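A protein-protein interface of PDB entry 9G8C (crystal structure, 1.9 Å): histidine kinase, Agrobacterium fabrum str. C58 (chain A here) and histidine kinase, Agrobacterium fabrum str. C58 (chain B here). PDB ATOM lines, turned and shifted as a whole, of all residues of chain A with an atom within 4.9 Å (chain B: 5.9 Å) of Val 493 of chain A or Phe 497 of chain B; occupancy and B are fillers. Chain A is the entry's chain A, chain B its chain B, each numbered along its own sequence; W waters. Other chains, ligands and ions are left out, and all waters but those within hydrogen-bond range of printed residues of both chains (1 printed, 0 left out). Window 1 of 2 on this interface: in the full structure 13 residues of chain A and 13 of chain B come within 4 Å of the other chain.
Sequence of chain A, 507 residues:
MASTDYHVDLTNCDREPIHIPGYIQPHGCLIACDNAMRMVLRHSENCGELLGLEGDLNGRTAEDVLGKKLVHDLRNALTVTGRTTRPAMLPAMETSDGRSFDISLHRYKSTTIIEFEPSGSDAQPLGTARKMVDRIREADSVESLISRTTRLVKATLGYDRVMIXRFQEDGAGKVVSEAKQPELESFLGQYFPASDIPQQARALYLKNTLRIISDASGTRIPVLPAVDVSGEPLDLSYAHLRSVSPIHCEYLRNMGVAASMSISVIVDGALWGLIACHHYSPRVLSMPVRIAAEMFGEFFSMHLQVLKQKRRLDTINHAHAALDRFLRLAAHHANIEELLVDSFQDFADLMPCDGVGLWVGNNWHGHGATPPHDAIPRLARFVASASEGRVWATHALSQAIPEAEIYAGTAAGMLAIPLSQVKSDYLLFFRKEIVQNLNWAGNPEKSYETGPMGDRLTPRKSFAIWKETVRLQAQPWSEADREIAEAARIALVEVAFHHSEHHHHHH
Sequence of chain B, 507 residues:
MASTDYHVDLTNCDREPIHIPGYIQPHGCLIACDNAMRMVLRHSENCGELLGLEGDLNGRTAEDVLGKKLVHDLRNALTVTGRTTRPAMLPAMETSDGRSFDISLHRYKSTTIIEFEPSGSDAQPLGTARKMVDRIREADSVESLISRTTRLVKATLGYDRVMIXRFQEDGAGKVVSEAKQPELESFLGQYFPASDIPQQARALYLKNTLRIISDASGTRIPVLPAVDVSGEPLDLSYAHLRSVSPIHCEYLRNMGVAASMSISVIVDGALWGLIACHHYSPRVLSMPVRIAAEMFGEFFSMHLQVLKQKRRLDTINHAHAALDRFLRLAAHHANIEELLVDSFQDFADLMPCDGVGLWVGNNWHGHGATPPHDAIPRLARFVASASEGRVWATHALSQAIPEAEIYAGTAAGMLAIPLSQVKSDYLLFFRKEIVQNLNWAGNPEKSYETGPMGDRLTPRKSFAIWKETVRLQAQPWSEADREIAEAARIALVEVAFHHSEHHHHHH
Printed residues of chain B within 4 Å of Ile 490 of chain A: Glu 494 (3.9 Å). Of the printed residues of chain B, Glu 494 of chain A touches Val 493. Of the printed residues of chain B, Phe 497 of chain A touches Val 493 (3.9 Å), Ala 496 (3.5 Å) and Phe 497 (3.7 Å). Of the printed residues of chain A, Val 493 of chain B touches Glu 494 and Phe 497. Val 495 of chain B touches none of the printed residues of chain A. Phe 497 of chain B touches just these residues of chain A: Val 493, Ala 496 and Phe 497. Ser 500 of chain B touches none of the printed residues of chain A. The nearest residue of chain B that does not touch Val 493 of chain A is Glu 494 of chain B (4.1 Å). The nearest printed residue of chain A that does not touch Phe 497 of chain B is Leu 492 of chain A (5.9 Å).
Ile 490 of chain A touches Glu 494 of chain B (CG1 to OE1, 3.9 Å). Val 493 of chain A touches Phe 497 of chain B. CG1 of Val 493 of chain B touches CG of Glu 494 of chain A, at 3.8 Å. CZ of Phe 497 of chain B touches CB of Ala 496 of chain A (3.5 Å). Phe 497 of chain A touches Val 493 of chain B. Phe 497 of chain A touches Ala 496 of chain B (CZ to CB, 3.5 Å). Phe 497 of chain B touches Phe 497 of chain A.
NH1 of Arg 489 of chain A is in salt-bridge range of OE2 of Glu 494 of chain B, 2.6 Å away.
Water W1 bridges OE2 of Glu 494 of chain B and NH2 of Arg 489 of chain A.
Of the 9 printed residues of chain A, 6 touch a printed residue of chain B. Hydrophobic or aromatic side chains of chain A that line the printed part of chain B: Ile 490, Val 493, Ala 496 and Phe 497. Hydrophobic or aromatic side chains of chain B within 4 Å of the printed part of chain A: Val 493, Ala 496 and Phe 497. Among the printed residues, 8 pairs touch across the chains.
The side-chain carboxylate (OE2) of Glu 494 of chain B sits at hydrogen-bond distance from a ring nitrogen (NE2) of His 498 of chain B (2.9 Å). The side-chain hydroxyl of Ser 500 of chain B lies within hydrogen-bond range of the backbone carbonyl oxygen of Phe 497 of chain B, at 2.7 Å.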
ATOM      1  N   ARG A 489      -3.336 -35.795 -12.840  1.00  0.00           N
ATOM      2  CA  ARG A 489      -3.663 -34.444 -13.379  1.00  0.00           C
ATOM      3  C   ARG A 489      -2.852 -33.382 -12.627  1.00  0.00           C
ATOM      4  O   ARG A 489      -2.270 -32.480 -13.271  1.00  0.00           O
ATOM      5  CB  ARG A 489      -5.146 -34.102 -13.213  1.00  0.00           C
ATOM      6  CG  ARG A 489      -5.534 -32.767 -13.849  1.00  0.00           C
ATOM      7  CD  ARG A 489      -6.994 -32.416 -13.638  1.00  0.00           C
ATOM      8  NE  ARG A 489      -7.286 -32.108 -12.246  1.00  0.00           N
ATOM      9  CZ  ARG A 489      -6.894 -30.999 -11.611  1.00  0.00           C
ATOM     10  NH1 ARG A 489      -6.192 -30.072 -12.235  1.00  0.00           N
ATOM     11  NH2 ARG A 489      -7.206 -30.820 -10.344  1.00  0.00           N
ATOM     12  N   ILE A 490      -2.813 -33.509 -11.304  1.00  0.00           N
ATOM     13  CA  ILE A 490      -2.143 -32.539 -10.386  1.00  0.00           C
ATOM     14  C   ILE A 490      -0.621 -32.633 -10.565  1.00  0.00           C
ATOM     15  O   ILE A 490       0.030 -31.580 -10.581  1.00  0.00           O
ATOM     16  CB  ILE A 490      -2.565 -32.807  -8.928  1.00  0.00           C
ATOM     17  CG1 ILE A 490      -3.972 -32.276  -8.647  1.00  0.00           C
ATOM     18  CG2 ILE A 490      -1.543 -32.247  -7.952  1.00  0.00           C
ATOM     19  CD1 ILE A 490      -4.574 -32.803  -7.359  1.00  0.00           C
ATOM     20  N   ALA A 491      -0.082 -33.846 -10.651  1.00  0.00           N
ATOM     21  CA  ALA A 491       1.375 -34.042 -10.822  1.00  0.00           C
ATOM     22  C   ALA A 491       1.829 -33.335 -12.106  1.00  0.00           C
ATOM     23  O   ALA A 491       2.913 -32.718 -12.094  1.00  0.00           O
ATOM     24  CB  ALA A 491       1.735 -35.497 -10.852  1.00  0.00           C
ATOM     25  N   LEU A 492       1.031 -33.415 -13.169  1.00  0.00           N
ATOM     26  CA  LEU A 492       1.357 -32.778 -14.470  1.00  0.00           C
ATOM     27  C   LEU A 492       1.259 -31.249 -14.362  1.00  0.00           C
ATOM     28  O   LEU A 492       2.113 -30.572 -14.959  1.00  0.00           O
ATOM     29  CB  LEU A 492       0.427 -33.350 -15.545  1.00  0.00           C
ATOM     30  CG  LEU A 492       0.619 -34.847 -15.787  1.00  0.00           C
ATOM     31  CD1 LEU A 492      -0.382 -35.375 -16.781  1.00  0.00           C
ATOM     32  CD2 LEU A 492       2.026 -35.151 -16.257  1.00  0.00           C
ATOM     33  N   VAL A 493       0.241 -30.742 -13.662  1.00  0.00           N
ATOM     34  CA  VAL A 493       0.135 -29.281 -13.374  1.00  0.00           C
ATOM     35  C   VAL A 493       1.442 -28.842 -12.712  1.00  0.00           C
ATOM     36  O   VAL A 493       2.026 -27.830 -13.149  1.00  0.00           O
ATOM     37  CB  VAL A 493      -1.088 -28.940 -12.510  1.00  0.00           C
ATOM     38  CG1 VAL A 493      -0.972 -27.546 -11.907  1.00  0.00           C
ATOM     39  CG2 VAL A 493      -2.371 -29.073 -13.311  1.00  0.00           C
ATOM     40  N   GLU A 494       1.902 -29.592 -11.715  1.00  0.00           N
ATOM     41  CA  GLU A 494       3.158 -29.269 -10.991  1.00  0.00           C
ATOM     42  C   GLU A 494       4.347 -29.295 -11.959  1.00  0.00           C
ATOM     43  O   GLU A 494       5.186 -28.374 -11.877  1.00  0.00           O
ATOM     44  CB  GLU A 494       3.452 -30.249  -9.866  1.00  0.00           C
ATOM     45  CG  GLU A 494       2.868 -29.858  -8.534  1.00  0.00           C
ATOM     46  CD  GLU A 494       3.719 -30.327  -7.369  1.00  0.00           C
ATOM     47  OE1 GLU A 494       3.345 -31.330  -6.781  1.00  0.00           O
ATOM     48  OE2 GLU A 494       4.766 -29.702  -7.086  1.00  0.00           O
ATOM     49  N   VAL A 495       4.454 -30.327 -12.799  1.00  0.00           N
ATOM     50  CA  VAL A 495       5.561 -30.411 -13.802  1.00  0.00           C
ATOM     51  C   VAL A 495       5.532 -29.143 -14.657  1.00  0.00           C
ATOM     52  O   VAL A 495       6.564 -28.481 -14.751  1.00  0.00           O
ATOM     53  CB  VAL A 495       5.465 -31.691 -14.653  1.00  0.00           C
ATOM     54  CG1 VAL A 495       6.363 -31.630 -15.883  1.00  0.00           C
ATOM     55  CG2 VAL A 495       5.789 -32.910 -13.815  1.00  0.00           C
ATOM     56  N   ALA A 496       4.376 -28.810 -15.221  1.00  0.00           N
ATOM     57  CA  ALA A 496       4.174 -27.663 -16.133  1.00  0.00           C
ATOM     58  C   ALA A 496       4.550 -26.354 -15.423  1.00  0.00           C
ATOM     59  O   ALA A 496       5.279 -25.547 -16.034  1.00  0.00           O
ATOM     60  CB  ALA A 496       2.753 -27.644 -16.617  1.00  0.00           C
ATOM     61  N   PHE A 497       4.111 -26.156 -14.171  1.00  0.00           N
ATOM     62  CA  PHE A 497       4.339 -24.894 -13.419  1.00  0.00           C
ATOM     63  C   PHE A 497       5.821 -24.729 -13.086  1.00  0.00           C
ATOM     64  O   PHE A 497       6.362 -23.633 -13.353  1.00  0.00           O
ATOM     65  CB  PHE A 497       3.518 -24.809 -12.128  1.00  0.00           C
ATOM     66  CG  PHE A 497       3.642 -23.470 -11.437  1.00  0.00           C
ATOM     67  CD1 PHE A 497       3.257 -22.304 -12.084  1.00  0.00           C
ATOM     68  CD2 PHE A 497       4.176 -23.368 -10.160  1.00  0.00           C
ATOM     69  CE1 PHE A 497       3.384 -21.069 -11.460  1.00  0.00           C
ATOM     70  CE2 PHE A 497       4.296 -22.132  -9.536  1.00  0.00           C
ATOM     71  CZ  PHE A 497       3.898 -20.988 -10.187  1.00  0.00           C
ATOM     72  N   LEU B 492      -2.024 -24.411  -4.145  1.00  0.00           N
ATOM     73  CA  LEU B 492      -1.448 -23.072  -4.445  1.00  0.00           C
ATOM     74  C   LEU B 492      -0.638 -23.134  -5.746  1.00  0.00           C
ATOM     75  O   LEU B 492      -0.761 -22.186  -6.546  1.00  0.00           O
ATOM     76  CB  LEU B 492      -0.624 -22.598  -3.244  1.00  0.00           C
ATOM     77  CG  LEU B 492      -1.475 -22.341  -1.998  1.00  0.00           C
ATOM     78  CD1 LEU B 492      -0.618 -22.120  -0.775  1.00  0.00           C
ATOM     79  CD2 LEU B 492      -2.394 -21.159  -2.218  1.00  0.00           C
ATOM     80  N   VAL B 493       0.137 -24.200  -5.945  1.00  0.00           N
ATOM     81  CA  VAL B 493       0.801 -24.450  -7.255  1.00  0.00           C
ATOM     82  C   VAL B 493      -0.276 -24.358  -8.337  1.00  0.00           C
ATOM     83  O   VAL B 493      -0.051 -23.673  -9.355  1.00  0.00           O
ATOM     84  CB  VAL B 493       1.527 -25.802  -7.308  1.00  0.00           C
ATOM     85  CG1 VAL B 493       1.902 -26.154  -8.743  1.00  0.00           C
ATOM     86  CG2 VAL B 493       2.759 -25.811  -6.417  1.00  0.00           C
ATOM     87  N   GLU B 494      -1.423 -24.986  -8.096  1.00  0.00           N
ATOM     88  CA  GLU B 494      -2.522 -25.078  -9.081  1.00  0.00           C
ATOM     89  C   GLU B 494      -3.126 -23.685  -9.303  1.00  0.00           C
ATOM     90  O   GLU B 494      -3.339 -23.305 -10.476  1.00  0.00           O
ATOM     91  CB  GLU B 494      -3.542 -26.122  -8.644  1.00  0.00           C
ATOM     92  CG  GLU B 494      -4.547 -26.391  -9.735  1.00  0.00           C
ATOM     93  CD  GLU B 494      -5.237 -27.743  -9.765  1.00  0.00           C
ATOM     94  OE1 GLU B 494      -5.065 -28.552  -8.830  1.00  0.00           O
ATOM     95  OE2 GLU B 494      -5.996 -27.941 -10.718  1.00  0.00           O
ATOM     96  N   VAL B 495      -3.370 -22.927  -8.233  1.00  0.00           N
ATOM     97  CA  VAL B 495      -3.873 -21.527  -8.356  1.00  0.00           C
ATOM     98  C   VAL B 495      -2.897 -20.707  -9.203  1.00  0.00           C
ATOM     99  O   VAL B 495      -3.372 -19.976 -10.086  1.00  0.00           O
ATOM    100  CB  VAL B 495      -4.104 -20.877  -6.981  1.00  0.00           C
ATOM    101  CG1 VAL B 495      -4.257 -19.368  -7.103  1.00  0.00           C
ATOM    102  CG2 VAL B 495      -5.305 -21.501  -6.298  1.00  0.00           C
ATOM    103  N   ALA B 496      -1.597 -20.813  -8.931  1.00  0.00           N
ATOM    104  CA  ALA B 496      -0.542 -20.018  -9.602  1.00  0.00           C
ATOM    105  C   ALA B 496      -0.475 -20.413 -11.086  1.00  0.00           C
ATOM    106  O   ALA B 496      -0.343 -19.511 -11.941  1.00  0.00           O
ATOM    107  CB  ALA B 496       0.784 -20.196  -8.910  1.00  0.00           C
ATOM    108  N   PHE B 497      -0.554 -21.712 -11.386  1.00  0.00           N
ATOM    109  CA  PHE B 497      -0.392 -22.232 -12.768  1.00  0.00           C
ATOM    110  C   PHE B 497      -1.576 -21.784 -13.624  1.00  0.00           C
ATOM    111  O   PHE B 497      -1.333 -21.235 -14.708  1.00  0.00           O
ATOM    112  CB  PHE B 497      -0.239 -23.755 -12.817  1.00  0.00           C
ATOM    113  CG  PHE B 497      -0.028 -24.272 -14.222  1.00  0.00           C
ATOM    114  CD1 PHE B 497       1.091 -23.893 -14.949  1.00  0.00           C
ATOM    115  CD2 PHE B 497      -0.960 -25.090 -14.837  1.00  0.00           C
ATOM    116  CE1 PHE B 497       1.277 -24.335 -16.253  1.00  0.00           C
ATOM    117  CE2 PHE B 497      -0.764 -25.546 -16.135  1.00  0.00           C
ATOM    118  CZ  PHE B 497       0.350 -25.163 -16.840  1.00  0.00           C
ATOM    119  N   HIS B 498      -2.809 -22.010 -13.164  1.00  0.00           N
ATOM    120  CA  HIS B 498      -4.039 -21.629 -13.906  1.00  0.00           C
ATOM    121  C   HIS B 498      -4.064 -20.109 -14.081  1.00  0.00           C
ATOM    122  O   HIS B 498      -4.466 -19.631 -15.170  1.00  0.00           O
ATOM    123  CB  HIS B 498      -5.299 -22.181 -13.236  1.00  0.00           C
ATOM    124  CG  HIS B 498      -5.287 -23.669 -13.135  1.00  0.00           C
ATOM    125  ND1 HIS B 498      -4.858 -24.483 -14.178  1.00  0.00           N
ATOM    126  CD2 HIS B 498      -5.646 -24.494 -12.129  1.00  0.00           C
ATOM    127  CE1 HIS B 498      -4.953 -25.746 -13.808  1.00  0.00           C
ATOM    128  NE2 HIS B 498      -5.426 -25.781 -12.549  1.00  0.00           N
ATOM    129  N   HIS B 499      -3.594 -19.374 -13.077  1.00  0.00           N
ATOM    130  CA  HIS B 499      -3.486 -17.894 -13.155  1.00  0.00           C
ATOM    131  C   HIS B 499      -2.550 -17.515 -14.312  1.00  0.00           C
ATOM    132  O   HIS B 499      -2.945 -16.666 -15.123  1.00  0.00           O
ATOM    133  CB  HIS B 499      -3.039 -17.293 -11.823  1.00  0.00           C
ATOM    134  CG  HIS B 499      -3.082 -15.805 -11.847  1.00  0.00           C
ATOM    135  ND1 HIS B 499      -4.267 -15.104 -11.648  1.00  0.00           N
ATOM    136  CD2 HIS B 499      -2.116 -14.891 -12.089  1.00  0.00           C
ATOM    137  CE1 HIS B 499      -4.020 -13.815 -11.748  1.00  0.00           C
ATOM    138  NE2 HIS B 499      -2.703 -13.654 -12.032  1.00  0.00           N
ATOM    139  N   SER B 500      -1.375 -18.145 -14.397  1.00  0.00           N
ATOM    140  CA  SER B 500      -0.381 -17.913 -15.484  1.00  0.00           C
ATOM    141  C   SER B 500      -0.983 -18.313 -16.845  1.00  0.00           C
ATOM    142  O   SER B 500      -0.761 -17.573 -17.808  1.00  0.00           O
ATOM    143  CB  SER B 500       0.920 -18.615 -15.215  1.00  0.00           C
ATOM    144  OG  SER B 500       0.848 -19.982 -15.589  1.00  0.00           O
ATOM    145  N   GLU B 501      -1.760 -19.402 -16.912  1.00  0.00           N
ATOM    146  CA  GLU B 501      -2.402 -19.915 -18.160  1.00  0.00           C
ATOM    147  C   GLU B 501      -3.392 -18.895 -18.732  1.00  0.00           C
ATOM    148  O   GLU B 501      -3.448 -18.753 -19.963  1.00  0.00           O
ATOM    149  CB  GLU B 501      -3.196 -21.196 -17.906  1.00  0.00           C
ATOM    150  CG  GLU B 501      -2.351 -22.444 -17.723  1.00  0.00           C
ATOM    151  CD  GLU B 501      -3.204 -23.683 -17.521  1.00  0.00           C
ATOM    152  OE1 GLU B 501      -3.022 -24.655 -18.286  1.00  0.00           O
ATOM    153  OE2 GLU B 501      -4.084 -23.654 -16.625  1.00  0.00           O
ATOM    154  N   HIS B 502      -4.184 -18.255 -17.870  1.00  0.00           N
ATOM    155  CA  HIS B 502      -5.377 -17.458 -18.265  1.00  0.00           C
ATOM    156  C   HIS B 502      -5.056 -15.953 -18.293  1.00  0.00           C
ATOM    157  O   HIS B 502      -5.942 -15.189 -18.710  1.00  0.00           O
ATOM    158  CB  HIS B 502      -6.566 -17.817 -17.363  1.00  0.00           C
ATOM    159  CG  HIS B 502      -7.094 -19.200 -17.579  1.00  0.00           C
ATOM    160  ND1 HIS B 502      -7.752 -19.572 -18.741  1.00  0.00           N
ATOM    161  CD2 HIS B 502      -7.080 -20.295 -16.786  1.00  0.00           C
ATOM    162  CE1 HIS B 502      -8.112 -20.837 -18.654  1.00  0.00           C
ATOM    163  NE2 HIS B 502      -7.711 -21.305 -17.461  1.00  0.00           N
HETATM  164  O   HOH W   1      -8.403 -27.744 -10.572  1.00  0.00           O
